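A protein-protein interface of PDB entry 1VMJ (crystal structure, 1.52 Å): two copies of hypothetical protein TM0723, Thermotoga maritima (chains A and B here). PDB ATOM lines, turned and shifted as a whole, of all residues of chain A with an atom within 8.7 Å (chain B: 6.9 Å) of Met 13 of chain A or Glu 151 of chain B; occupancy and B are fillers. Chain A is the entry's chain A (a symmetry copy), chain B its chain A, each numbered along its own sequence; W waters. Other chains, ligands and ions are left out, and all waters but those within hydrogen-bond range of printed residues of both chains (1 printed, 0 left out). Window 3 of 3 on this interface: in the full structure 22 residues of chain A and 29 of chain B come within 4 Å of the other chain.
The side-chain carboxylate (OE1) of Glu 48 of chain B lies within salt-bridge range of the side-chain amino group (NZ) of Lys 147 of chain A (2.7 Å).
The backbone carbonyl oxygen of Ile 118 of chain B lies within hydrogen-bond range of the side-chain amino group of Lys 147 of chain A, 3.1 Å away.
The backbone carbonyl oxygen of Gly 150 of chain B lies within hydrogen-bond range of the backbone NH of Lys 14 of chain B (2.8 Å).
NZ of Lys 47 of chain B lies within salt-bridge range of OE2 of Glu 48 of chain B.
The chain-end carboxylate of Glu 151 of chain B is in hydrogen-bond range of the backbone NH of Lys 47 of chain B (3.1 Å).
The chain-end carboxylate (O) of Glu 151 of chain B is in hydrogen-bond range of the backbone NH (N) of Glu 48 of chain B, 2.9 Å away.
The backbone NH (N) of Ile 118 of chain B is in hydrogen-bond range of the backbone carbonyl oxygen (O) of Gly 49 of chain B (2.9 Å).
The backbone NH (N) of Leu 50 of chain B lies within hydrogen-bond range of the backbone carbonyl oxygen (O) of Ile 149 of chain B, at 3.0 Å.
Met 13 of chain A touches Glu 48 of chain B (CE to O, 3.5 Å).
Gly 150 of chain B touches Met 13 of chain A.
Met 13 of chain A touches Glu 151 of chain B (CE to N, 3.8 Å).
CB of Glu 48 of chain B touches OG of Ser 15 of chain A, 3.6 Å away.
Lys 147 of chain A touches Gly 49 of chain B (CE to O, 3.8 Å).
CG of Lys 147 of chain A touches CD2 of Leu 50 of chain B (3.998 Å).
Ile 149 of chain A touches Leu 50 of chain B (CD1 to CG, 3.9 Å).
Ile 149 of chain A touches Ile 149 of chain B (CD1 to CG1, 3.9 Å).
Met 13 of chain A touches just these residues of chain B: Glu 48, Gly 150 and Glu 151.
Of the printed residues of chain A, Glu 151 of chain B touches Met 13 (3.8 Å).
Gly 150 of chain B touches just one residue of chain A: Met 13 (3.7 Å).
Of the printed residues of chain B, Lys 147 of chain A touches Glu 48, Gly 49, Leu 50 and Ile 118.
Of the printed residues of chain A, Ile 118 of chain B touches Lys 147.
Of the printed residues of chain A, Gly 49 of chain B touches Lys 147 (3.8 Å).
Ile 46 of chain A touches none of the printed residues of chain B.
Gly 45 of chain B touches none of the printed residues of chain A.
The nearest residue of chain A that does not touch Glu 151 of chain B is Ile 149 of chain A (6.9 Å).
Of the 12 printed residues of chain A, 4 touch a printed residue of chain B.
Hydrophobic or aromatic side chains of chain A that line the printed part of chain B: Met 13 and Ile 149.
Hydrophobic or aromatic side chains of chain B within 4 Å of the printed part of chain A: Leu 50 and Ile 149.
Among the printed residues, 10 pairs touch across the chains.
Among the printed residues, Asp or Glu carboxylates within 4 Å of a Lys or Arg side-chain nitrogen of the other chain: Lys 147 of chain A with Glu 48 of chain B.
Met 13 of chain A touches Glu 48 of chain B, but with the chains exchanged Glu 48 of chain A does not touch Met 13 of chain B (10.2 Å).
Met 13 of chain A touches Gly 150 of chain B, but with the chains exchanged Gly 150 of chain A does not touch Met 13 of chain B (8.2 Å).
Met 13 of chain A touches Glu 151 of chain B, but with the chains exchanged Glu 151 of chain A does not touch Met 13 of chain B (9.4 Å).
Ile 149 of chain B touches its own counterpart, Ile 149 of chain A.
Water W1 lies within hydrogen-bond range of NZ of Lys 147 of chain A, OG of Ser 15 of chain A and OE1 of Glu 48 of chain B.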
ATOM      1  N   MET A  13      14.099  -0.851 -31.090  1.00  0.00           N
ATOM      2  CA  MET A  13      14.572  -2.050 -30.312  1.00  0.00           C
ATOM      3  C   MET A  13      15.057  -3.125 -31.246  1.00  0.00           C
ATOM      4  O   MET A  13      14.406  -3.437 -32.243  1.00  0.00           O
ATOM      5  CB  MET A  13      13.452  -2.656 -29.474  1.00  0.00           C
ATOM      6  CG  MET A  13      13.963  -3.711 -28.491  1.00  0.00           C
ATOM      7  SD  MET A  13      12.665  -4.773 -27.834  1.00  0.00           S
ATOM      8  CE  MET A  13      12.382  -5.942 -29.208  1.00  0.00           C
ATOM      9  N   LYS A  14      16.163  -3.754 -30.890  1.00  0.00           N
ATOM     10  CA  LYS A  14      16.679  -4.817 -31.704  1.00  0.00           C
ATOM     11  C   LYS A  14      16.210  -6.138 -31.119  1.00  0.00           C
ATOM     12  O   LYS A  14      16.008  -6.273 -29.905  1.00  0.00           O
ATOM     13  CB  LYS A  14      18.200  -4.811 -31.716  1.00  0.00           C
ATOM     14  CG  LYS A  14      18.828  -3.567 -32.283  1.00  0.00           C
ATOM     15  CD  LYS A  14      20.333  -3.609 -32.128  1.00  0.00           C
ATOM     16  CE  LYS A  14      20.976  -2.283 -32.536  1.00  0.00           C
ATOM     17  N   SER A  15      16.055  -7.115 -32.001  1.00  0.00           N
ATOM     18  CA  SER A  15      15.826  -8.480 -31.575  1.00  0.00           C
ATOM     19  C   SER A  15      16.563  -9.417 -32.489  1.00  0.00           C
ATOM     20  O   SER A  15      16.891  -9.084 -33.641  1.00  0.00           O
ATOM     21  CB  SER A  15      14.349  -8.856 -31.533  1.00  0.00           C
ATOM     22  OG  SER A  15      13.820  -9.096 -32.801  1.00  0.00           O
ATOM     23  N   TYR A  16      16.864 -10.588 -31.951  1.00  0.00           N
ATOM     24  CA  TYR A  16      17.638 -11.588 -32.629  1.00  0.00           C
ATOM     25  C   TYR A  16      17.108 -12.938 -32.232  1.00  0.00           C
ATOM     26  O   TYR A  16      16.785 -13.152 -31.058  1.00  0.00           O
ATOM     27  CB  TYR A  16      19.112 -11.448 -32.226  1.00  0.00           C
ATOM     28  CG  TYR A  16      19.990 -12.545 -32.769  1.00  0.00           C
ATOM     29  CD1 TYR A  16      20.147 -13.746 -32.087  1.00  0.00           C
ATOM     30  CD2 TYR A  16      20.632 -12.392 -33.974  1.00  0.00           C
ATOM     31  CE1 TYR A  16      20.932 -14.747 -32.604  1.00  0.00           C
ATOM     32  CE2 TYR A  16      21.456 -13.392 -34.505  1.00  0.00           C
ATOM     33  CZ  TYR A  16      21.597 -14.571 -33.793  1.00  0.00           C
ATOM     34  OH  TYR A  16      22.377 -15.590 -34.257  1.00  0.00           O
ATOM     35  N   ILE A  46      23.615  -6.442 -30.618  1.00  0.00           N
ATOM     36  CA  ILE A  46      23.006  -5.874 -29.431  1.00  0.00           C
ATOM     37  C   ILE A  46      24.075  -5.565 -28.388  1.00  0.00           C
ATOM     38  O   ILE A  46      24.900  -6.413 -28.073  1.00  0.00           O
ATOM     39  CB  ILE A  46      21.916  -6.812 -28.883  1.00  0.00           C
ATOM     40  CG1 ILE A  46      20.749  -6.827 -29.877  1.00  0.00           C
ATOM     41  CG2 ILE A  46      21.462  -6.402 -27.457  1.00  0.00           C
ATOM     42  CD1 ILE A  46      19.747  -7.938 -29.689  1.00  0.00           C
ATOM     43  N   GLU A  48      23.307  -3.905 -25.167  1.00  0.00           N
ATOM     44  CA  GLU A  48      22.719  -4.072 -23.828  1.00  0.00           C
ATOM     45  C   GLU A  48      21.370  -4.744 -23.984  1.00  0.00           C
ATOM     46  O   GLU A  48      20.548  -4.320 -24.795  1.00  0.00           O
ATOM     47  CB  GLU A  48      22.509  -2.709 -23.192  1.00  0.00           C
ATOM     48  CG  GLU A  48      23.767  -1.840 -23.156  1.00  0.00           C
ATOM     49  CD  GLU A  48      24.846  -2.389 -22.241  1.00  0.00           C
ATOM     50  OE1 GLU A  48      24.502  -3.123 -21.296  1.00  0.00           O
ATOM     51  OE2 GLU A  48      26.062  -2.081 -22.461  1.00  0.00           O
ATOM     52  N   GLY A  49      21.133  -5.799 -23.221  1.00  0.00           N
ATOM     53  CA  GLY A  49      19.886  -6.510 -23.382  1.00  0.00           C
ATOM     54  C   GLY A  49      19.789  -7.742 -22.516  1.00  0.00           C
ATOM     55  O   GLY A  49      20.524  -7.883 -21.549  1.00  0.00           O
ATOM     56  N   LYS A 147      17.002 -16.237 -28.095  1.00  0.00           N
ATOM     57  CA  LYS A 147      16.316 -15.009 -28.367  1.00  0.00           C
ATOM     58  C   LYS A 147      16.946 -13.882 -27.569  1.00  0.00           C
ATOM     59  O   LYS A 147      17.153 -14.012 -26.381  1.00  0.00           O
ATOM     60  CB  LYS A 147      14.827 -15.146 -27.997  1.00  0.00           C
ATOM     61  CG  LYS A 147      13.937 -13.921 -28.359  1.00  0.00           C
ATOM     62  CD  LYS A 147      13.589 -13.860 -29.811  1.00  0.00           C
ATOM     63  CE  LYS A 147      12.580 -12.738 -30.083  1.00  0.00           C
ATOM     64  NZ  LYS A 147      12.081 -12.777 -31.516  1.00  0.00           N
ATOM     65  N   ILE A 148      17.300 -12.796 -28.258  1.00  0.00           N
ATOM     66  CA  ILE A 148      17.925 -11.642 -27.627  1.00  0.00           C
ATOM     67  C   ILE A 148      17.142 -10.408 -27.939  1.00  0.00           C
ATOM     68  O   ILE A 148      16.738 -10.207 -29.073  1.00  0.00           O
ATOM     69  CB  ILE A 148      19.379 -11.432 -28.094  1.00  0.00           C
ATOM     70  CG1 ILE A 148      20.119 -12.778 -28.142  1.00  0.00           C
ATOM     71  CG2 ILE A 148      20.073 -10.458 -27.150  1.00  0.00           C
ATOM     72  CD1 ILE A 148      21.523 -12.686 -28.714  1.00  0.00           C
ATOM     73  N   ILE A 149      16.868  -9.612 -26.931  1.00  0.00           N
ATOM     74  CA  ILE A 149      16.259  -8.311 -27.157  1.00  0.00           C
ATOM     75  C   ILE A 149      17.087  -7.230 -26.481  1.00  0.00           C
ATOM     76  O   ILE A 149      17.724  -7.471 -25.438  1.00  0.00           O
ATOM     77  CB  ILE A 149      14.781  -8.218 -26.711  1.00  0.00           C
ATOM     78  CG1 ILE A 149      14.625  -8.353 -25.211  1.00  0.00           C
ATOM     79  CG2 ILE A 149      13.932  -9.269 -27.405  1.00  0.00           C
ATOM     80  CD1 ILE A 149      13.223  -7.922 -24.756  1.00  0.00           C
ATOM     81  N   GLY A 150      17.104  -6.048 -27.071  1.00  0.00           N
ATOM     82  CA  GLY A 150      17.775  -4.936 -26.419  1.00  0.00           C
ATOM     83  C   GLY A 150      18.120  -3.888 -27.424  1.00  0.00           C
ATOM     84  O   GLY A 150      17.442  -3.778 -28.442  1.00  0.00           O
ATOM     85  N   GLU A 151      19.195  -3.157 -27.156  1.00  0.00           N
ATOM     86  CA  GLU A 151      19.718  -2.165 -28.091  1.00  0.00           C
ATOM     87  C   GLU A 151      21.225  -2.282 -28.136  1.00  0.00           C
ATOM     88  O   GLU A 151      21.850  -2.369 -27.094  1.00  0.00           O
ATOM     89  CB  GLU A 151      19.296  -0.764 -27.665  1.00  0.00           C
ATOM     90  OXT GLU A 151      21.847  -2.239 -29.195  1.00  0.00           O
ATOM     91  N   MET B  13       9.103   1.556 -26.774  1.00  0.00           N
ATOM     92  CA  MET B  13       8.991   0.126 -26.318  1.00  0.00           C
ATOM     93  C   MET B  13       7.603  -0.159 -25.816  1.00  0.00           C
ATOM     94  O   MET B  13       7.033   0.623 -25.055  1.00  0.00           O
ATOM     95  CB  MET B  13       9.953  -0.179 -25.176  1.00  0.00           C
ATOM     96  CG  MET B  13      10.038  -1.675 -24.867  1.00  0.00           C
ATOM     97  SD  MET B  13      10.767  -2.039 -23.260  1.00  0.00           S
ATOM     98  CE  MET B  13       9.384  -1.706 -22.116  1.00  0.00           C
ATOM     99  N   LYS B  14       7.077  -1.319 -26.172  1.00  0.00           N
ATOM    100  CA  LYS B  14       5.771  -1.688 -25.709  1.00  0.00           C
ATOM    101  C   LYS B  14       5.930  -2.584 -24.493  1.00  0.00           C
ATOM    102  O   LYS B  14       6.912  -3.324 -24.358  1.00  0.00           O
ATOM    103  CB  LYS B  14       5.008  -2.459 -26.776  1.00  0.00           C
ATOM    104  CG  LYS B  14       4.754  -1.702 -28.050  1.00  0.00           C
ATOM    105  CD  LYS B  14       4.109  -2.598 -29.085  1.00  0.00           C
ATOM    106  CE  LYS B  14       4.001  -1.902 -30.443  1.00  0.00           C
ATOM    107  N   SER B  44      -1.523  -7.805 -26.826  1.00  0.00           N
ATOM    108  CA  SER B  44      -0.408  -6.902 -26.593  1.00  0.00           C
ATOM    109  C   SER B  44       0.020  -6.141 -27.822  1.00  0.00           C
ATOM    110  O   SER B  44       0.610  -5.057 -27.705  1.00  0.00           O
ATOM    111  CB  SER B  44       0.795  -7.664 -26.052  1.00  0.00           C
ATOM    112  OG  SER B  44       1.436  -8.438 -27.062  1.00  0.00           O
ATOM    113  N   GLY B  45      -0.186  -6.752 -28.983  1.00  0.00           N
ATOM    114  CA  GLY B  45       0.311  -6.189 -30.241  1.00  0.00           C
ATOM    115  C   GLY B  45       1.818  -6.251 -30.418  1.00  0.00           C
ATOM    116  O   GLY B  45       2.357  -5.711 -31.386  1.00  0.00           O
ATOM    117  N   ILE B  46       2.516  -6.885 -29.495  1.00  0.00           N
ATOM    118  CA  ILE B  46       3.960  -6.990 -29.573  1.00  0.00           C
ATOM    119  C   ILE B  46       4.356  -8.018 -30.627  1.00  0.00           C
ATOM    120  O   ILE B  46       3.853  -9.135 -30.628  1.00  0.00           O
ATOM    121  CB  ILE B  46       4.551  -7.320 -28.191  1.00  0.00           C
ATOM    122  CG1 ILE B  46       4.358  -6.102 -27.280  1.00  0.00           C
ATOM    123  CG2 ILE B  46       6.041  -7.748 -28.284  1.00  0.00           C
ATOM    124  CD1 ILE B  46       4.560  -6.351 -25.807  1.00  0.00           C
ATOM    125  N   LYS B  47       5.262  -7.634 -31.530  1.00  0.00           N
ATOM    126  CA  LYS B  47       5.694  -8.517 -32.598  1.00  0.00           C
ATOM    127  C   LYS B  47       6.910  -9.341 -32.185  1.00  0.00           C
ATOM    128  O   LYS B  47       6.968 -10.530 -32.476  1.00  0.00           O
ATOM    129  CB  LYS B  47       6.015  -7.746 -33.875  1.00  0.00           C
ATOM    130  CG  LYS B  47       6.425  -8.698 -34.988  1.00  0.00           C
ATOM    131  CD  LYS B  47       6.513  -8.045 -36.333  1.00  0.00           C
ATOM    132  CE  LYS B  47       7.309  -8.914 -37.270  1.00  0.00           C
ATOM    133  NZ  LYS B  47       8.700  -8.941 -36.808  1.00  0.00           N
ATOM    134  N   GLU B  48       7.882  -8.691 -31.540  1.00  0.00           N
ATOM    135  CA  GLU B  48       9.142  -9.330 -31.123  1.00  0.00           C
ATOM    136  C   GLU B  48       9.425  -8.928 -29.689  1.00  0.00           C
ATOM    137  O   GLU B  48       9.376  -7.747 -29.348  1.00  0.00           O
ATOM    138  CB  GLU B  48      10.278  -8.831 -31.997  1.00  0.00           C
ATOM    139  CG  GLU B  48      10.027  -8.996 -33.497  1.00  0.00           C
ATOM    140  CD  GLU B  48       9.978 -10.447 -33.939  1.00  0.00           C
ATOM    141  OE1 GLU B  48      10.586 -11.293 -33.257  1.00  0.00           O
ATOM    142  OE2 GLU B  48       9.327 -10.755 -34.988  1.00  0.00           O
ATOM    143  N   GLY B  49       9.711  -9.901 -28.839  1.00  0.00           N
ATOM    144  CA  GLY B  49       9.924  -9.571 -27.449  1.00  0.00           C
ATOM    145  C   GLY B  49      10.150 -10.782 -26.579  1.00  0.00           C
ATOM    146  O   GLY B  49      10.475 -11.853 -27.074  1.00  0.00           O
ATOM    147  N   LEU B  50       9.996 -10.584 -25.273  1.00  0.00           N
ATOM    148  CA  LEU B  50      10.082 -11.643 -24.281  1.00  0.00           C
ATOM    149  C   LEU B  50       8.857 -11.554 -23.405  1.00  0.00           C
ATOM    150  O   LEU B  50       8.460 -10.457 -23.004  1.00  0.00           O
ATOM    151  CB  LEU B  50      11.319 -11.512 -23.404  1.00  0.00           C
ATOM    152  CG  LEU B  50      12.687 -11.692 -24.054  1.00  0.00           C
ATOM    153  CD1 LEU B  50      13.791 -11.450 -23.039  1.00  0.00           C
ATOM    154  CD2 LEU B  50      12.819 -13.077 -24.614  1.00  0.00           C
ATOM    155  N   ILE B 118       8.831 -14.088 -27.925  1.00  0.00           N
ATOM    156  CA  ILE B 118       7.776 -13.680 -28.845  1.00  0.00           C
ATOM    157  C   ILE B 118       8.437 -13.361 -30.165  1.00  0.00           C
ATOM    158  O   ILE B 118       9.321 -12.500 -30.239  1.00  0.00           O
ATOM    159  CB  ILE B 118       6.989 -12.463 -28.310  1.00  0.00           C
ATOM    160  CG1 ILE B 118       6.444 -12.751 -26.903  1.00  0.00           C
ATOM    161  CG2 ILE B 118       5.881 -12.073 -29.265  1.00  0.00           C
ATOM    162  CD1 ILE B 118       5.660 -14.000 -26.772  1.00  0.00           C
ATOM    163  N   ILE B 149       7.452  -7.582 -22.838  1.00  0.00           N
ATOM    164  CA  ILE B 149       8.097  -6.370 -23.317  1.00  0.00           C
ATOM    165  C   ILE B 149       8.637  -6.595 -24.720  1.00  0.00           C
ATOM    166  O   ILE B 149       9.030  -7.719 -25.082  1.00  0.00           O
ATOM    167  CB  ILE B 149       9.214  -5.837 -22.388  1.00  0.00           C
ATOM    168  CG1 ILE B 149      10.394  -6.782 -22.309  1.00  0.00           C
ATOM    169  CG2 ILE B 149       8.682  -5.573 -20.989  1.00  0.00           C
ATOM    170  CD1 ILE B 149      11.614  -6.097 -21.673  1.00  0.00           C
ATOM    171  N   GLY B 150       8.644  -5.544 -25.522  1.00  0.00           N
ATOM    172  CA  GLY B 150       9.255  -5.655 -26.836  1.00  0.00           C
ATOM    173  C   GLY B 150       8.726  -4.589 -27.736  1.00  0.00           C
ATOM    174  O   GLY B 150       8.321  -3.535 -27.255  1.00  0.00           O
ATOM    175  N   GLU B 151       8.689  -4.887 -29.030  1.00  0.00           N
ATOM    176  CA  GLU B 151       8.102  -3.990 -30.021  1.00  0.00           C
ATOM    177  C   GLU B 151       7.272  -4.804 -30.988  1.00  0.00           C
ATOM    178  O   GLU B 151       7.731  -5.833 -31.450  1.00  0.00           O
ATOM    179  CB  GLU B 151       9.198  -3.227 -30.757  1.00  0.00           C
ATOM    180  OXT GLU B 151       6.163  -4.431 -31.363  1.00  0.00           O
HETATM  181  O   HOH W   1      13.890 -11.985 -33.427  1.00  0.00           O
